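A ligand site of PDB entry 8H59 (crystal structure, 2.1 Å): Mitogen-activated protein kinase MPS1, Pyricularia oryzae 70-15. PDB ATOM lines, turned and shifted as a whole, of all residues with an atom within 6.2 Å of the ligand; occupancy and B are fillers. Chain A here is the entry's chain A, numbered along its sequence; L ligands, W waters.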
ATOM      1  N   LEU A  25      -7.216  -4.453  -9.051  1.00  0.00           N
ATOM      2  CA  LEU A  25      -7.552  -3.394  -8.108  1.00  0.00           C
ATOM      3  C   LEU A  25      -7.783  -3.912  -6.709  1.00  0.00           C
ATOM      4  O   LEU A  25      -7.310  -3.311  -5.750  1.00  0.00           O
ATOM      5  CB  LEU A  25      -8.814  -2.647  -8.560  1.00  0.00           C
ATOM      6  CG  LEU A  25      -8.674  -1.905  -9.883  1.00  0.00           C
ATOM      7  CD1 LEU A  25      -9.969  -1.194 -10.254  1.00  0.00           C
ATOM      8  CD2 LEU A  25      -7.503  -0.928  -9.815  1.00  0.00           C
ATOM      9  N   GLY A  26      -8.488  -5.026  -6.548  1.00  0.00           N
ATOM     10  CA  GLY A  26      -8.734  -5.536  -5.218  1.00  0.00           C
ATOM     11  C   GLY A  26      -9.624  -6.746  -5.270  1.00  0.00           C
ATOM     12  O   GLY A  26     -10.137  -7.115  -6.325  1.00  0.00           O
ATOM     13  N   GLN A  27      -9.797  -7.345  -4.095  1.00  0.00           N
ATOM     14  CA  GLN A  27     -10.610  -8.544  -3.898  1.00  0.00           C
ATOM     15  C   GLN A  27     -11.248  -8.438  -2.537  1.00  0.00           C
ATOM     16  O   GLN A  27     -10.620  -7.983  -1.585  1.00  0.00           O
ATOM     17  CB  GLN A  27      -9.740  -9.797  -3.974  1.00  0.00           C
ATOM     18  CG  GLN A  27     -10.434 -11.062  -3.512  1.00  0.00           C
ATOM     19  CD  GLN A  27      -9.568 -12.287  -3.762  1.00  0.00           C
ATOM     20  OE1 GLN A  27      -8.328 -12.198  -3.815  1.00  0.00           O
ATOM     21  NE2 GLN A  27     -10.218 -13.449  -3.922  1.00  0.00           N
ATOM     22  N   GLY A  28     -12.507  -8.850  -2.438  1.00  0.00           N
ATOM     23  CA  GLY A  28     -13.219  -8.818  -1.174  1.00  0.00           C
ATOM     24  C   GLY A  28     -13.991 -10.103  -0.983  1.00  0.00           C
ATOM     25  O   GLY A  28     -13.768 -11.074  -1.703  1.00  0.00           O
ATOM     26  N   TYR A  30     -16.923 -10.648  -1.868  1.00  0.00           N
ATOM     27  CA  TYR A  30     -17.944 -10.795  -2.891  1.00  0.00           C
ATOM     28  C   TYR A  30     -17.375 -10.942  -4.286  1.00  0.00           C
ATOM     29  O   TYR A  30     -18.147 -11.180  -5.217  1.00  0.00           O
ATOM     30  CB  TYR A  30     -18.910  -9.590  -2.837  1.00  0.00           C
ATOM     31  CG  TYR A  30     -19.313  -9.279  -1.396  1.00  0.00           C
ATOM     32  CD1 TYR A  30     -19.819 -10.276  -0.600  1.00  0.00           C
ATOM     33  CD2 TYR A  30     -19.135  -8.018  -0.839  1.00  0.00           C
ATOM     34  CE1 TYR A  30     -20.142 -10.050   0.719  1.00  0.00           C
ATOM     35  CE2 TYR A  30     -19.477  -7.771   0.494  1.00  0.00           C
ATOM     36  CZ  TYR A  30     -19.968  -8.805   1.260  1.00  0.00           C
ATOM     37  OH  TYR A  30     -20.317  -8.638   2.573  1.00  0.00           O
ATOM     38  N   GLY A  31     -16.060 -10.827  -4.470  1.00  0.00           N
ATOM     39  CA  GLY A  31     -15.488 -11.003  -5.793  1.00  0.00           C
ATOM     40  C   GLY A  31     -14.190 -10.252  -5.931  1.00  0.00           C
ATOM     41  O   GLY A  31     -13.556  -9.880  -4.955  1.00  0.00           O
ATOM     42  N   ILE A  32     -13.811 -10.031  -7.197  1.00  0.00           N
ATOM     43  CA  ILE A  32     -12.547  -9.390  -7.520  1.00  0.00           C
ATOM     44  C   ILE A  32     -12.807  -8.285  -8.527  1.00  0.00           C
ATOM     45  O   ILE A  32     -13.766  -8.331  -9.306  1.00  0.00           O
ATOM     46  CB  ILE A  32     -11.525 -10.382  -8.090  1.00  0.00           C
ATOM     47  CG1 ILE A  32     -12.124 -11.147  -9.263  1.00  0.00           C
ATOM     48  CG2 ILE A  32     -11.057 -11.356  -7.026  1.00  0.00           C
ATOM     49  CD1 ILE A  32     -11.248 -12.312  -9.722  1.00  0.00           C
ATOM     50  N   VAL A  33     -11.931  -7.278  -8.512  1.00  0.00           N
ATOM     51  CA  VAL A  33     -12.089  -6.107  -9.364  1.00  0.00           C
ATOM     52  C   VAL A  33     -10.780  -5.812 -10.090  1.00  0.00           C
ATOM     53  O   VAL A  33      -9.710  -5.790  -9.462  1.00  0.00           O
ATOM     54  CB  VAL A  33     -12.532  -4.859  -8.582  1.00  0.00           C
ATOM     55  CG1 VAL A  33     -12.925  -3.743  -9.586  1.00  0.00           C
ATOM     56  CG2 VAL A  33     -13.658  -5.194  -7.641  1.00  0.00           C
ATOM     57  N   ALA A  46     -13.892   0.041 -14.603  1.00  0.00           N
ATOM     58  CA  ALA A  46     -13.681  -0.972 -13.570  1.00  0.00           C
ATOM     59  C   ALA A  46     -14.575  -2.171 -13.841  1.00  0.00           C
ATOM     60  O   ALA A  46     -15.784  -2.019 -14.048  1.00  0.00           O
ATOM     61  CB  ALA A  46     -13.978  -0.399 -12.187  1.00  0.00           C
ATOM     62  N   LYS A  48     -15.960  -5.687 -12.315  1.00  0.00           N
ATOM     63  CA  LYS A  48     -16.192  -6.358 -11.044  1.00  0.00           C
ATOM     64  C   LYS A  48     -16.782  -7.747 -11.308  1.00  0.00           C
ATOM     65  O   LYS A  48     -17.851  -7.888 -11.919  1.00  0.00           O
ATOM     66  CB  LYS A  48     -17.060  -5.396 -10.219  1.00  0.00           C
ATOM     67  CG  LYS A  48     -17.804  -5.894  -9.076  1.00  0.00           C
ATOM     68  CD  LYS A  48     -18.784  -4.750  -8.575  1.00  0.00           C
ATOM     69  CE  LYS A  48     -18.086  -3.563  -8.049  1.00  0.00           C
ATOM     70  NZ  LYS A  48     -19.047  -2.497  -7.557  1.00  0.00           N
ATOM     71  N   LYS A  49     -16.037  -8.765 -10.931  1.00  0.00           N
ATOM     72  CA  LYS A  49     -16.523 -10.130 -11.035  1.00  0.00           C
ATOM     73  C   LYS A  49     -17.128 -10.522  -9.700  1.00  0.00           C
ATOM     74  O   LYS A  49     -16.408 -10.802  -8.746  1.00  0.00           O
ATOM     75  CB  LYS A  49     -15.402 -11.088 -11.410  1.00  0.00           C
ATOM     76  CG  LYS A  49     -15.861 -12.529 -11.489  1.00  0.00           C
ATOM     77  CD  LYS A  49     -14.703 -13.486 -11.624  1.00  0.00           C
ATOM     78  CE  LYS A  49     -15.177 -14.872 -12.054  1.00  0.00           C
ATOM     79  NZ  LYS A  49     -14.063 -15.903 -11.948  1.00  0.00           N
ATOM     80  N   VAL A  50     -18.453 -10.557  -9.658  1.00  0.00           N
ATOM     81  CA  VAL A  50     -19.167 -11.001  -8.468  1.00  0.00           C
ATOM     82  C   VAL A  50     -19.154 -12.513  -8.466  1.00  0.00           C
ATOM     83  O   VAL A  50     -19.581 -13.162  -9.425  1.00  0.00           O
ATOM     84  CB  VAL A  50     -20.594 -10.429  -8.437  1.00  0.00           C
ATOM     85  CG1 VAL A  50     -21.255 -10.708  -7.089  1.00  0.00           C
ATOM     86  CG2 VAL A  50     -20.586  -8.928  -8.737  1.00  0.00           C
ATOM     87  N   THR A  51     -18.694 -13.086  -7.372  1.00  0.00           N
ATOM     88  CA  THR A  51     -18.132 -14.422  -7.330  1.00  0.00           C
ATOM     89  C   THR A  51     -18.973 -15.337  -6.455  1.00  0.00           C
ATOM     90  O   THR A  51     -19.578 -14.894  -5.475  1.00  0.00           O
ATOM     91  CB  THR A  51     -16.695 -14.281  -6.837  1.00  0.00           C
ATOM     92  OG1 THR A  51     -15.864 -15.094  -7.651  1.00  0.00           O
ATOM     93  CG2 THR A  51     -16.561 -14.633  -5.376  1.00  0.00           C
ATOM     94  N   ARG A  62     -27.337 -10.476  -2.013  1.00  0.00           N
ATOM     95  CA  ARG A  62     -26.505  -9.278  -2.078  1.00  0.00           C
ATOM     96  C   ARG A  62     -26.211  -8.912  -3.524  1.00  0.00           C
ATOM     97  O   ARG A  62     -26.239  -7.731  -3.894  1.00  0.00           O
ATOM     98  CB  ARG A  62     -25.195  -9.507  -1.311  1.00  0.00           C
ATOM     99  CG  ARG A  62     -24.417  -8.238  -0.934  1.00  0.00           C
ATOM    100  CD  ARG A  62     -22.899  -8.421  -1.108  1.00  0.00           C
ATOM    101  NE  ARG A  62     -22.602  -8.779  -2.475  1.00  0.00           N
ATOM    102  CZ  ARG A  62     -22.284  -7.915  -3.421  1.00  0.00           C
ATOM    103  NH1 ARG A  62     -22.000  -6.653  -3.135  1.00  0.00           N
ATOM    104  NH2 ARG A  62     -22.329  -8.296  -4.696  1.00  0.00           N
ATOM    105  N   GLU A  66     -27.255  -5.377  -5.238  1.00  0.00           N
ATOM    106  CA  GLU A  66     -26.310  -4.451  -5.852  1.00  0.00           C
ATOM    107  C   GLU A  66     -26.656  -4.197  -7.314  1.00  0.00           C
ATOM    108  O   GLU A  66     -26.641  -3.044  -7.779  1.00  0.00           O
ATOM    109  CB  GLU A  66     -24.887  -5.007  -5.700  1.00  0.00           C
ATOM    110  CG  GLU A  66     -23.874  -4.216  -6.499  1.00  0.00           C
ATOM    111  CD  GLU A  66     -22.439  -4.588  -6.201  1.00  0.00           C
ATOM    112  OE1 GLU A  66     -22.179  -5.763  -5.838  1.00  0.00           O
ATOM    113  OE2 GLU A  66     -21.565  -3.687  -6.342  1.00  0.00           O
ATOM    114  N   THR A  80     -20.891   6.245  -8.551  1.00  0.00           N
ATOM    115  CA  THR A  80     -20.331   5.346  -9.531  1.00  0.00           C
ATOM    116  C   THR A  80     -21.417   4.863 -10.480  1.00  0.00           C
ATOM    117  O   THR A  80     -22.468   4.394 -10.046  1.00  0.00           O
ATOM    118  CB  THR A  80     -19.694   4.180  -8.780  1.00  0.00           C
ATOM    119  OG1 THR A  80     -19.183   3.255  -9.719  1.00  0.00           O
ATOM    120  CG2 THR A  80     -20.734   3.410  -7.971  1.00  0.00           C
ATOM    121  N   LEU A  98     -19.877  -6.815 -13.610  1.00  0.00           N
ATOM    122  CA  LEU A  98     -20.388  -5.458 -13.671  1.00  0.00           C
ATOM    123  C   LEU A  98     -19.270  -4.546 -14.178  1.00  0.00           C
ATOM    124  O   LEU A  98     -18.121  -4.666 -13.736  1.00  0.00           O
ATOM    125  CB  LEU A  98     -20.897  -4.993 -12.311  1.00  0.00           C
ATOM    126  CG  LEU A  98     -21.579  -6.040 -11.457  1.00  0.00           C
ATOM    127  CD1 LEU A  98     -22.009  -5.480 -10.093  1.00  0.00           C
ATOM    128  CD2 LEU A  98     -22.776  -6.607 -12.185  1.00  0.00           C
ATOM    129  N   GLU A 100     -18.257  -0.787 -14.399  1.00  0.00           N
ATOM    130  CA  GLU A 100     -18.534   0.464 -13.723  1.00  0.00           C
ATOM    131  C   GLU A 100     -17.461   1.504 -14.042  1.00  0.00           C
ATOM    132  O   GLU A 100     -16.330   1.171 -14.413  1.00  0.00           O
ATOM    133  CB  GLU A 100     -18.562   0.260 -12.212  1.00  0.00           C
ATOM    134  CG  GLU A 100     -19.858   0.133 -11.593  1.00  0.00           C
ATOM    135  CD  GLU A 100     -19.791  -0.104 -10.092  1.00  0.00           C
ATOM    136  OE1 GLU A 100     -19.864   0.851  -9.290  1.00  0.00           O
ATOM    137  OE2 GLU A 100     -19.734  -1.286  -9.740  1.00  0.00           O
ATOM    138  N   GLU A 101     -17.869   2.771 -13.950  1.00  0.00           N
ATOM    139  CA  GLU A 101     -16.990   3.928 -14.092  1.00  0.00           C
ATOM    140  C   GLU A 101     -15.745   3.747 -13.234  1.00  0.00           C
ATOM    141  O   GLU A 101     -15.847   3.471 -12.044  1.00  0.00           O
ATOM    142  CB  GLU A 101     -17.776   5.162 -13.676  1.00  0.00           C
ATOM    143  CG  GLU A 101     -17.191   6.525 -13.877  1.00  0.00           C
ATOM    144  CD  GLU A 101     -18.181   7.596 -13.391  1.00  0.00           C
ATOM    145  OE1 GLU A 101     -19.242   7.235 -12.775  1.00  0.00           O
ATOM    146  OE2 GLU A 101     -17.944   8.795 -13.646  1.00  0.00           O
ATOM    147  N   LEU A 102     -14.586   3.934 -13.847  1.00  0.00           N
ATOM    148  CA  LEU A 102     -13.324   3.712 -13.148  1.00  0.00           C
ATOM    149  C   LEU A 102     -12.864   4.944 -12.357  1.00  0.00           C
ATOM    150  O   LEU A 102     -12.897   6.064 -12.857  1.00  0.00           O
ATOM    151  CB  LEU A 102     -12.244   3.330 -14.149  1.00  0.00           C
ATOM    152  CG  LEU A 102     -10.860   3.000 -13.589  1.00  0.00           C
ATOM    153  CD1 LEU A 102     -10.805   1.771 -12.717  1.00  0.00           C
ATOM    154  CD2 LEU A 102      -9.899   2.868 -14.784  1.00  0.00           C
ATOM    155  N   MET A 103     -12.337   4.745 -11.146  1.00  0.00           N
ATOM    156  CA  MET A 103     -11.857   5.823 -10.250  1.00  0.00           C
ATOM    157  C   MET A 103     -10.471   5.414  -9.707  1.00  0.00           C
ATOM    158  O   MET A 103     -10.323   4.271  -9.342  1.00  0.00           O
ATOM    159  CB  MET A 103     -12.853   6.041  -9.115  1.00  0.00           C
ATOM    160  CG  MET A 103     -14.194   6.566  -9.578  1.00  0.00           C
ATOM    161  SD  MET A 103     -14.104   8.187 -10.315  1.00  0.00           S
ATOM    162  CE  MET A 103     -14.335   9.207  -8.875  1.00  0.00           C
ATOM    163  N   GLU A 104      -9.473   6.291  -9.753  1.00  0.00           N
ATOM    164  CA  GLU A 104      -8.073   6.004  -9.361  1.00  0.00           C
ATOM    165  C   GLU A 104      -7.792   5.829  -7.864  1.00  0.00           C
ATOM    166  O   GLU A 104      -7.200   4.831  -7.539  1.00  0.00           O
ATOM    167  CB  GLU A 104      -7.194   7.112  -9.901  1.00  0.00           C
ATOM    168  CG  GLU A 104      -5.814   7.111  -9.306  1.00  0.00           C
ATOM    169  CD  GLU A 104      -4.810   7.916 -10.110  1.00  0.00           C
ATOM    170  OE1 GLU A 104      -5.177   9.002 -10.567  1.00  0.00           O
ATOM    171  OE2 GLU A 104      -3.696   7.429 -10.291  1.00  0.00           O
ATOM    172  N   CYS A 105      -8.268   6.681  -6.967  1.00  0.00           N
ATOM    173  CA  CYS A 105      -8.050   6.465  -5.518  1.00  0.00           C
ATOM    174  C   CYS A 105      -9.394   6.339  -4.788  1.00  0.00           C
ATOM    175  O   CYS A 105     -10.432   6.223  -5.450  1.00  0.00           O
ATOM    176  CB  CYS A 105      -7.219   7.623  -4.969  1.00  0.00           C
ATOM    177  SG  CYS A 105      -5.699   7.927  -5.906  1.00  0.00           S
ATOM    178  N   ASP A 106      -9.338   6.149  -3.474  1.00  0.00           N
ATOM    179  CA  ASP A 106     -10.478   6.293  -2.575  1.00  0.00           C
ATOM    180  C   ASP A 106     -10.055   7.201  -1.420  1.00  0.00           C
ATOM    181  O   ASP A 106      -8.860   7.473  -1.220  1.00  0.00           O
ATOM    182  CB  ASP A 106     -10.955   4.943  -2.096  1.00  0.00           C
ATOM    183  CG  ASP A 106      -9.887   4.182  -1.318  1.00  0.00           C
ATOM    184  OD1 ASP A 106      -9.520   4.620  -0.239  1.00  0.00           O
ATOM    185  OD2 ASP A 106      -9.443   3.109  -1.726  1.00  0.00           O
ATOM    186  N   LYS A 147     -18.259   5.161   4.295  1.00  0.00           N
ATOM    187  CA  LYS A 147     -16.955   5.270   4.950  1.00  0.00           C
ATOM    188  C   LYS A 147     -15.916   5.694   3.918  1.00  0.00           C
ATOM    189  O   LYS A 147     -16.154   5.590   2.716  1.00  0.00           O
ATOM    190  CB  LYS A 147     -16.552   3.962   5.609  1.00  0.00           C
ATOM    191  CG  LYS A 147     -16.386   2.874   4.632  1.00  0.00           C
ATOM    192  CD  LYS A 147     -16.357   1.501   5.334  1.00  0.00           C
ATOM    193  CE  LYS A 147     -16.383   0.377   4.253  1.00  0.00           C
ATOM    194  NZ  LYS A 147     -16.299  -0.994   4.878  1.00  0.00           N
ATOM    195  N   GLY A 149     -13.519   4.346   2.621  1.00  0.00           N
ATOM    196  CA  GLY A 149     -13.184   3.301   1.676  1.00  0.00           C
ATOM    197  C   GLY A 149     -14.147   3.156   0.493  1.00  0.00           C
ATOM    198  O   GLY A 149     -13.734   2.672  -0.567  1.00  0.00           O
ATOM    199  N   ASN A 150     -15.420   3.545   0.651  1.00  0.00           N
ATOM    200  CA  ASN A 150     -16.365   3.433  -0.481  1.00  0.00           C
ATOM    201  C   ASN A 150     -16.555   4.803  -1.160  1.00  0.00           C
ATOM    202  O   ASN A 150     -17.494   4.999  -1.948  1.00  0.00           O
ATOM    203  CB  ASN A 150     -17.763   2.975  -0.052  1.00  0.00           C
ATOM    204  CG  ASN A 150     -18.246   3.664   1.186  1.00  0.00           C
ATOM    205  OD1 ASN A 150     -18.162   4.910   1.356  1.00  0.00           O
ATOM    206  ND2 ASN A 150     -18.805   2.896   2.019  1.00  0.00           N
ATOM    207  N   LEU A 152     -14.981   6.954  -3.670  1.00  0.00           N
ATOM    208  CA  LEU A 152     -13.951   6.916  -4.710  1.00  0.00           C
ATOM    209  C   LEU A 152     -13.603   8.308  -5.225  1.00  0.00           C
ATOM    210  O   LEU A 152     -14.461   9.180  -5.370  1.00  0.00           O
ATOM    211  CB  LEU A 152     -14.406   6.042  -5.873  1.00  0.00           C
ATOM    212  CG  LEU A 152     -14.848   4.621  -5.489  1.00  0.00           C
ATOM    213  CD1 LEU A 152     -15.003   3.772  -6.717  1.00  0.00           C
ATOM    214  CD2 LEU A 152     -13.896   3.922  -4.527  1.00  0.00           C
ATOM    215  N   VAL A 153     -12.326   8.513  -5.510  1.00  0.00           N
ATOM    216  CA  VAL A 153     -11.825   9.857  -5.816  1.00  0.00           C
ATOM    217  C   VAL A 153     -10.891   9.733  -6.999  1.00  0.00           C
ATOM    218  O   VAL A 153     -10.155   8.738  -7.084  1.00  0.00           O
ATOM    219  CB  VAL A 153     -11.097  10.479  -4.616  1.00  0.00           C
ATOM    220  CG1 VAL A 153     -10.586  11.904  -4.984  1.00  0.00           C
ATOM    221  CG2 VAL A 153     -12.052  10.514  -3.396  1.00  0.00           C
ATOM    222  N   CYS A 162     -19.778   4.563  -3.919  1.00  0.00           N
ATOM    223  CA  CYS A 162     -19.885   3.226  -4.478  1.00  0.00           C
ATOM    224  C   CYS A 162     -20.371   2.261  -3.405  1.00  0.00           C
ATOM    225  O   CYS A 162     -20.494   2.621  -2.240  1.00  0.00           O
ATOM    226  CB  CYS A 162     -18.538   2.725  -5.067  1.00  0.00           C
ATOM    227  SG  CYS A 162     -17.268   2.087  -3.916  1.00  0.00           S
ATOM    228  N   ASP A 163     -20.639   1.028  -3.857  1.00  0.00           N
ATOM    229  CA  ASP A 163     -20.962  -0.131  -3.031  1.00  0.00           C
ATOM    230  C   ASP A 163     -22.341  -0.065  -2.377  1.00  0.00           C
ATOM    231  O   ASP A 163     -22.484   0.364  -1.226  1.00  0.00           O
ATOM    232  CB  ASP A 163     -19.923  -0.347  -1.942  1.00  0.00           C
ATOM    233  CG  ASP A 163     -19.962  -1.765  -1.406  1.00  0.00           C
ATOM    234  OD1 ASP A 163     -20.995  -2.422  -1.592  1.00  0.00           O
ATOM    235  OD2 ASP A 163     -18.986  -2.223  -0.791  1.00  0.00           O
ATOM    236  N   PHE A 164     -23.354  -0.507  -3.120  1.00  0.00           N
ATOM    237  CA  PHE A 164     -24.731  -0.592  -2.648  1.00  0.00           C
ATOM    238  C   PHE A 164     -25.066  -1.964  -2.066  1.00  0.00           C
ATOM    239  O   PHE A 164     -26.247  -2.251  -1.865  1.00  0.00           O
ATOM    240  CB  PHE A 164     -25.671  -0.251  -3.810  1.00  0.00           C
ATOM    241  CG  PHE A 164     -25.686   1.198  -4.125  1.00  0.00           C
ATOM    242  CD1 PHE A 164     -26.476   2.062  -3.389  1.00  0.00           C
ATOM    243  CD2 PHE A 164     -24.909   1.713  -5.169  1.00  0.00           C
ATOM    244  CE1 PHE A 164     -26.481   3.402  -3.660  1.00  0.00           C
ATOM    245  CE2 PHE A 164     -24.920   3.044  -5.450  1.00  0.00           C
ATOM    246  CZ  PHE A 164     -25.697   3.906  -4.669  1.00  0.00           C
ATOM    247  N   GLY A 165     -24.066  -2.783  -1.778  1.00  0.00           N
ATOM    248  CA  GLY A 165     -24.354  -4.147  -1.355  1.00  0.00           C
ATOM    249  C   GLY A 165     -25.030  -4.235  -0.004  1.00  0.00           C
ATOM    250  O   GLY A 165     -25.762  -5.198   0.273  1.00  0.00           O
HETATM  251  C1  LIG L   1     -15.329  -0.473  -0.104  1.00  0.00           C
HETATM  252  C2  LIG L   1     -15.764  -1.433  -2.358  1.00  0.00           C
HETATM  253  C3  LIG L   1     -16.566  -2.150  -3.475  1.00  0.00           C
HETATM  254  C4  LIG L   1     -16.946  -0.947  -5.609  1.00  0.00           C
HETATM  255  C5  LIG L   1     -16.296  -0.247  -6.769  1.00  0.00           C
HETATM  256  C6  LIG L   1     -14.345   0.594  -7.726  1.00  0.00           C
HETATM  257  C7  LIG L   1     -15.078   1.219  -8.703  1.00  0.00           C
HETATM  258  C8  LIG L   1     -14.412   1.990  -9.707  1.00  0.00           C
HETATM  259  C9  LIG L   1     -12.322   1.396  -8.820  1.00  0.00           C
HETATM  260  C10 LIG L   1     -12.931   0.655  -7.825  1.00  0.00           C
HETATM  261  C11 LIG L   1     -11.980  -0.020  -6.841  1.00  0.00           C
HETATM  262  C12 LIG L   1     -12.038  -1.378  -6.597  1.00  0.00           C
HETATM  263  C13 LIG L   1     -11.170  -1.986  -5.708  1.00  0.00           C
HETATM  264  C14 LIG L   1     -12.113  -3.760  -4.466  1.00  0.00           C
HETATM  265  C15 LIG L   1     -10.210  -1.212  -5.044  1.00  0.00           C
HETATM  266  C16 LIG L   1     -10.154   0.168  -5.284  1.00  0.00           C
HETATM  267  C17 LIG L   1     -11.030   0.772  -6.206  1.00  0.00           C
HETATM  268  C18 LIG L   1      -9.974   2.859  -5.914  1.00  0.00           C
HETATM  269  C19 LIG L   1     -16.513   1.186  -8.686  1.00  0.00           C
HETATM  270  C20 LIG L   1     -17.106   0.439  -7.676  1.00  0.00           C
HETATM  271  C21 LIG L   1     -16.344  -3.645  -3.353  1.00  0.00           C
HETATM  272  C22 LIG L   1     -17.457  -4.400  -4.070  1.00  0.00           C
HETATM  273  C23 LIG L   1     -18.830  -4.155  -4.138  1.00  0.00           C
HETATM  274  C24 LIG L   1     -18.374  -5.971  -5.344  1.00  0.00           C
HETATM  275  C25 LIG L   1     -17.177  -5.536  -4.822  1.00  0.00           C
HETATM  276  C26 LIG L   1     -15.978  -6.227  -5.091  1.00  0.00           C
HETATM  277  C27 LIG L   1     -15.998  -7.356  -5.906  1.00  0.00           C
HETATM  278  C28 LIG L   1     -17.219  -7.806  -6.421  1.00  0.00           C
HETATM  279  C29 LIG L   1     -18.408  -7.128  -6.148  1.00  0.00           C
HETATM  280  F1  LIG L   1     -12.143  -5.115  -4.364  1.00  0.00           F
HETATM  281  F2  LIG L   1     -13.393  -3.328  -4.624  1.00  0.00           F
HETATM  282  F3  LIG L   1     -11.606  -3.201  -3.350  1.00  0.00           F
HETATM  283  N1  LIG L   1     -16.272  -1.085  -1.035  1.00  0.00           N
HETATM  284  N2  LIG L   1     -16.040  -1.594  -4.701  1.00  0.00           N
HETATM  285  N3  LIG L   1     -14.973  -0.144  -6.763  1.00  0.00           N
HETATM  286  N4  LIG L   1     -13.062   2.034  -9.731  1.00  0.00           N
HETATM  287  N5  LIG L   1     -19.348  -5.118  -4.912  1.00  0.00           N
HETATM  288  O1  LIG L   1     -11.278  -3.386  -5.521  1.00  0.00           O
HETATM  289  O2  LIG L   1     -11.024   2.138  -6.506  1.00  0.00           O
HETATM  290  O3  LIG L   1     -18.107  -0.804  -5.369  1.00  0.00           O
HETATM  291  O4  LIG L   1     -14.606  -1.152  -2.530  1.00  0.00           O
HETATM  292  O   HOH W   1     -13.654  -4.124  -0.766  1.00  0.00           O
HETATM  293  O   HOH W   2     -20.710   0.768  -6.838  1.00  0.00           O
HETATM  294  O   HOH W   3     -18.467  -1.019   1.536  1.00  0.00           O
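The side-chain sulfur (SG) of Cys 162 lies within hydrogen-bond range of an oxygen (O3) of the ligand, at 3.3 Å.
The backbone NH of Gly 26 sits close to an oxygen (O1) of the ligand (3.4 Å).
N1 of the ligand lies within hydrogen-bond range of OD2 of Asp 163 (3.0 Å).
The backbone NH (N) of Met 103 lies within hydrogen-bond range of a nitrogen (N4) of the ligand (3.1 Å).
N of Asp 163 lies within hydrogen-bond range of O3 of the ligand, at 3.5 Å.
An oxygen (O3) of the ligand sits at hydrogen-bond distance from the side-chain amino group (NZ) of Lys 48 (2.9 Å).
The side-chain carboxylate of Glu 66 sits at hydrogen-bond distance from a nitrogen (N5) of the ligand, at 3.0 Å.
O of Val 153 sits at hydrogen-bond distance from N of Cys 105 (2.8 Å).
O of Val 33 lies within hydrogen-bond range of N of Leu 25.
The backbone carbonyl oxygen (O) of Tyr 30 sits at hydrogen-bond distance from the backbone NH (N) of Thr 51 (2.9 Å).
OG1 of Thr 80 lies within hydrogen-bond range of OE1 of Glu 100, 2.5 Å away.
The side-chain carboxylate (OE2) of Glu 100 lies within salt-bridge range of the side-chain amino group (NZ) of Lys 48.
The backbone NH (N) of Ala 46 sits at hydrogen-bond distance from the backbone carbonyl oxygen (O) of Glu 100, at 2.7 Å.
The side-chain carboxylate of Glu 66 is in salt-bridge range of the side-chain amino group of Lys 48 (3.0 Å).
The backbone carbonyl oxygen (O) of Gly 26 is in hydrogen-bond range of the backbone NH (N) of Val 33.
The backbone NH (N) of Gln 27 lies close to a fluorine (F1) of the ligand, 3.2 Å away.
Merely in contact with the ligand: Leu 25, Tyr 30, Gly 31, Ile 32, Val 33, Ala 46, Lys 49, Val 50, Arg 62, Thr 80, Glu 100, Glu 101, Leu 102, Glu 104, Cys 105, Gly 149 and Leu 152.
The nearest printed residue that does not touch the ligand is Asn 150 (4.1 Å).
Water W2 lies within hydrogen-bond range of the side-chain carboxylate of Glu 100 (2.6 Å), the backbone NH of Asp 163 (3.0 Å) and an oxygen (O3) of the ligand (3.4 Å).
Water W3 bridges OD2 of Asp 163 (2.7 Å) and N1 of the ligand (3.4 Å).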
